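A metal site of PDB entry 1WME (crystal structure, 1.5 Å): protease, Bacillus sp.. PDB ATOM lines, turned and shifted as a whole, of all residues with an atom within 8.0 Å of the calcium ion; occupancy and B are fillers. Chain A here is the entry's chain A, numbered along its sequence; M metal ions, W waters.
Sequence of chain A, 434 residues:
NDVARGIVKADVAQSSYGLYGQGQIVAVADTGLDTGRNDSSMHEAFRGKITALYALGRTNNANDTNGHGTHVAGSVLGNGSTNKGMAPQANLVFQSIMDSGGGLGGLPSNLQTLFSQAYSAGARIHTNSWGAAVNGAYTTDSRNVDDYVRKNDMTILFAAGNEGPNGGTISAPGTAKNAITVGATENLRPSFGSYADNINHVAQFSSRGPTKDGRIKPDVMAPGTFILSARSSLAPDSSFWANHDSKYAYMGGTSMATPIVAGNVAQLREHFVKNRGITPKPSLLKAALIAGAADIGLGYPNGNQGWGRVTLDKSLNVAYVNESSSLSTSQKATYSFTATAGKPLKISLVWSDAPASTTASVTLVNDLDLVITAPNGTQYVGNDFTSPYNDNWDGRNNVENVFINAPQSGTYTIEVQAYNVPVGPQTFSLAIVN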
ATOM      1  N   GLU A 186      13.568  -1.188   4.624  1.00  0.00           N
ATOM      2  CA  GLU A 186      12.777  -1.772   5.694  1.00  0.00           C
ATOM      3  C   GLU A 186      12.349  -0.756   6.733  1.00  0.00           C
ATOM      4  O   GLU A 186      13.106   0.158   7.034  1.00  0.00           O
ATOM      5  CB  GLU A 186      13.590  -2.894   6.392  1.00  0.00           C
ATOM      6  CG  GLU A 186      13.863  -4.041   5.412  1.00  0.00           C
ATOM      7  CD  GLU A 186      14.597  -5.204   6.051  1.00  0.00           C
ATOM      8  OE1 GLU A 186      14.916  -6.191   5.345  1.00  0.00           O
ATOM      9  OE2 GLU A 186      14.956  -5.147   7.268  1.00  0.00           O
ATOM     10  N   ASN A 187      11.125  -0.949   7.259  1.00  0.00           N
ATOM     11  CA  ASN A 187      10.774  -0.219   8.480  1.00  0.00           C
ATOM     12  C   ASN A 187      11.461  -0.856   9.677  1.00  0.00           C
ATOM     13  O   ASN A 187      11.951  -2.001   9.558  1.00  0.00           O
ATOM     14  CB  ASN A 187       9.237  -0.273   8.645  1.00  0.00           C
ATOM     15  CG  ASN A 187       8.606   0.882   9.353  1.00  0.00           C
ATOM     16  OD1 ASN A 187       9.303   1.857   9.590  1.00  0.00           O
ATOM     17  ND2 ASN A 187       7.336   0.829   9.705  1.00  0.00           N
ATOM     18  N   GLY A 193      10.303  -9.450  12.648  1.00  0.00           N
ATOM     19  CA  GLY A 193      11.225 -10.341  11.946  1.00  0.00           C
ATOM     20  C   GLY A 193      12.134  -9.660  10.939  1.00  0.00           C
ATOM     21  O   GLY A 193      12.317  -8.448  10.920  1.00  0.00           O
ATOM     22  N   SER A 194      12.727 -10.497  10.092  1.00  0.00           N
ATOM     23  CA  SER A 194      13.807 -10.005   9.265  1.00  0.00           C
ATOM     24  C   SER A 194      13.334  -9.022   8.190  1.00  0.00           C
ATOM     25  O   SER A 194      14.257  -8.400   7.632  1.00  0.00           O
ATOM     26  CB  SER A 194      14.589 -11.166   8.622  1.00  0.00           C
ATOM     27  OG  SER A 194      13.744 -11.799   7.723  1.00  0.00           O
ATOM     28  N   TYR A 195      12.035  -8.898   7.936  1.00  0.00           N
ATOM     29  CA  TYR A 195      11.631  -7.914   6.919  1.00  0.00           C
ATOM     30  C   TYR A 195      11.564  -6.549   7.552  1.00  0.00           C
ATOM     31  O   TYR A 195      11.296  -5.615   6.782  1.00  0.00           O
ATOM     32  CB  TYR A 195      10.265  -8.271   6.301  1.00  0.00           C
ATOM     33  CG  TYR A 195      10.401  -9.121   5.065  1.00  0.00           C
ATOM     34  CD1 TYR A 195      10.525 -10.499   5.232  1.00  0.00           C
ATOM     35  CD2 TYR A 195      10.400  -8.596   3.798  1.00  0.00           C
ATOM     36  CE1 TYR A 195      10.650 -11.319   4.127  1.00  0.00           C
ATOM     37  CE2 TYR A 195      10.525  -9.408   2.663  1.00  0.00           C
ATOM     38  CZ  TYR A 195      10.649 -10.761   2.856  1.00  0.00           C
ATOM     39  OH  TYR A 195      10.772 -11.621   1.786  1.00  0.00           O
ATOM     40  N   ALA A 196      11.804  -6.403   8.849  1.00  0.00           N
ATOM     41  CA  ALA A 196      11.624  -5.074   9.465  1.00  0.00           C
ATOM     42  C   ALA A 196      12.655  -4.876  10.547  1.00  0.00           C
ATOM     43  O   ALA A 196      12.329  -4.398  11.664  1.00  0.00           O
ATOM     44  CB  ALA A 196      10.214  -4.890  10.026  1.00  0.00           C
ATOM     45  N   ASP A 197      13.923  -5.201  10.232  1.00  0.00           N
ATOM     46  CA  ASP A 197      14.916  -5.141  11.306  1.00  0.00           C
ATOM     47  C   ASP A 197      16.077  -4.211  11.035  1.00  0.00           C
ATOM     48  O   ASP A 197      16.853  -3.989  11.983  1.00  0.00           O
ATOM     49  CB  ASP A 197      15.483  -6.537  11.677  1.00  0.00           C
ATOM     50  CG  ASP A 197      16.201  -7.242  10.555  1.00  0.00           C
ATOM     51  OD1 ASP A 197      16.217  -6.719   9.403  1.00  0.00           O
ATOM     52  OD2 ASP A 197      16.781  -8.346  10.769  1.00  0.00           O
ATOM     53  N   ASN A 198      16.221  -3.631   9.843  1.00  0.00           N
ATOM     54  CA  ASN A 198      17.380  -2.732   9.653  1.00  0.00           C
ATOM     55  C   ASN A 198      16.972  -1.659   8.662  1.00  0.00           C
ATOM     56  O   ASN A 198      16.607  -1.989   7.522  1.00  0.00           O
ATOM     57  CB  ASN A 198      18.571  -3.523   9.124  1.00  0.00           C
ATOM     58  CG  ASN A 198      19.827  -2.679   9.024  1.00  0.00           C
ATOM     59  OD1 ASN A 198      19.773  -1.486   8.740  1.00  0.00           O
ATOM     60  ND2 ASN A 198      20.983  -3.299   9.272  1.00  0.00           N
ATOM     61  N   ILE A 199      16.996  -0.403   9.080  1.00  0.00           N
ATOM     62  CA  ILE A 199      16.517   0.665   8.204  1.00  0.00           C
ATOM     63  C   ILE A 199      17.418   0.873   6.996  1.00  0.00           C
ATOM     64  O   ILE A 199      16.978   1.609   6.072  1.00  0.00           O
ATOM     65  CB  ILE A 199      16.362   2.015   8.963  1.00  0.00           C
ATOM     66  CG1 ILE A 199      17.725   2.563   9.421  1.00  0.00           C
ATOM     67  CG2 ILE A 199      15.317   1.833  10.068  1.00  0.00           C
ATOM     68  CD1 ILE A 199      17.632   3.998   9.927  1.00  0.00           C
ATOM     69  N   ASN A 200      18.611   0.275   7.014  1.00  0.00           N
ATOM     70  CA  ASN A 200      19.539   0.387   5.907  1.00  0.00           C
ATOM     71  C   ASN A 200      19.525  -0.862   5.017  1.00  0.00           C
ATOM     72  O   ASN A 200      20.448  -1.105   4.220  1.00  0.00           O
ATOM     73  CB  ASN A 200      20.974   0.666   6.406  1.00  0.00           C
ATOM     74  CG  ASN A 200      21.090   2.025   7.041  1.00  0.00           C
ATOM     75  OD1 ASN A 200      20.751   3.002   6.361  1.00  0.00           O
ATOM     76  ND2 ASN A 200      21.584   2.122   8.283  1.00  0.00           N
ATOM     77  N   HIS A 201      18.506  -1.687   5.143  1.00  0.00           N
ATOM     78  CA  HIS A 201      18.316  -2.867   4.288  1.00  0.00           C
ATOM     79  C   HIS A 201      17.351  -2.508   3.162  1.00  0.00           C
ATOM     80  O   HIS A 201      16.291  -1.951   3.479  1.00  0.00           O
ATOM     81  CB  HIS A 201      17.699  -4.075   4.990  1.00  0.00           C
ATOM     82  CG  HIS A 201      18.662  -4.882   5.815  1.00  0.00           C
ATOM     83  ND1 HIS A 201      18.282  -6.006   6.534  1.00  0.00           N
ATOM     84  CD2 HIS A 201      20.014  -4.704   6.004  1.00  0.00           C
ATOM     85  CE1 HIS A 201      19.355  -6.507   7.154  1.00  0.00           C
ATOM     86  NE2 HIS A 201      20.432  -5.735   6.866  1.00  0.00           N
ATOM     87  N   VAL A 202      17.683  -2.846   1.911  1.00  0.00           N
ATOM     88  CA  VAL A 202      16.662  -2.773   0.873  1.00  0.00           C
ATOM     89  C   VAL A 202      15.736  -3.954   1.033  1.00  0.00           C
ATOM     90  O   VAL A 202      16.161  -5.110   1.245  1.00  0.00           O
ATOM     91  CB  VAL A 202      17.331  -2.874  -0.500  1.00  0.00           C
ATOM     92  CG1 VAL A 202      16.271  -2.860  -1.607  1.00  0.00           C
ATOM     93  CG2 VAL A 202      18.327  -1.744  -0.687  1.00  0.00           C
ATOM     94  N   ALA A 203      14.426  -3.742   0.932  1.00  0.00           N
ATOM     95  CA  ALA A 203      13.480  -4.843   1.088  1.00  0.00           C
ATOM     96  C   ALA A 203      13.745  -5.859  -0.023  1.00  0.00           C
ATOM     97  O   ALA A 203      13.981  -5.437  -1.166  1.00  0.00           O
ATOM     98  CB  ALA A 203      12.057  -4.316   1.080  1.00  0.00           C
ATOM     99  N   GLN A 204      13.718  -7.166   0.274  1.00  0.00           N
ATOM    100  CA  GLN A 204      14.144  -8.149  -0.727  1.00  0.00           C
ATOM    101  C   GLN A 204      13.324  -8.022  -2.005  1.00  0.00           C
ATOM    102  O   GLN A 204      13.856  -8.178  -3.104  1.00  0.00           O
ATOM    103  CB  GLN A 204      14.009  -9.577  -0.168  1.00  0.00           C
ATOM    104  CG  GLN A 204      14.857 -10.581  -0.940  1.00  0.00           C
ATOM    105  CD  GLN A 204      15.011 -11.941  -0.304  1.00  0.00           C
ATOM    106  OE1 GLN A 204      15.684 -12.834  -0.839  1.00  0.00           O
ATOM    107  NE2 GLN A 204      14.417 -12.132   0.880  1.00  0.00           N
ATOM    108  N   THR A 225       8.158  -1.854   4.534  1.00  0.00           N
ATOM    109  CA  THR A 225       7.723  -3.139   5.106  1.00  0.00           C
ATOM    110  C   THR A 225       6.957  -2.893   6.406  1.00  0.00           C
ATOM    111  O   THR A 225       7.344  -1.940   7.086  1.00  0.00           O
ATOM    112  CB  THR A 225       8.915  -4.067   5.375  1.00  0.00           C
ATOM    113  OG1 THR A 225       9.799  -3.451   6.307  1.00  0.00           O
ATOM    114  CG2 THR A 225       9.725  -4.319   4.101  1.00  0.00           C
HETATM  115 CA    CA M   1      16.198  -7.251   7.161  1.00  0.00          CA
HETATM  116  O   HOH W   1      17.528  -8.976   8.220  1.00  0.00           O
HETATM  117  O   HOH W   2      16.622  -8.724   5.341  1.00  0.00           O
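The side-chain carboxylate (OE2) of Glu 186 sits close to the backbone NH (N) of Asn 198 (3.2 Å).
A ring nitrogen (NE2) of His 201 lies within hydrogen-bond range of the side-chain amide nitrogen of Asn 198.
Within 4 Å of the calcium ion: Glu 186, Ser 194, Asp 197 and His 201.
The calcium ion is bound by the side-chain carboxylate (OD1) of Asp 197 (2.3 Å), the backbone carbonyl oxygen (O) of Ser 194 (2.3 Å), water W2 (2.4 Å), water W1 (2.4 Å), the side-chain carboxylate (OE2) of Glu 186 (2.4 Å), the side-chain carboxylate (OE1) of Glu 186 (2.5 Å) and a ring nitrogen (ND1) of His 201 (2.5 Å).
The calcium ion has seven donor atoms within binding distance.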
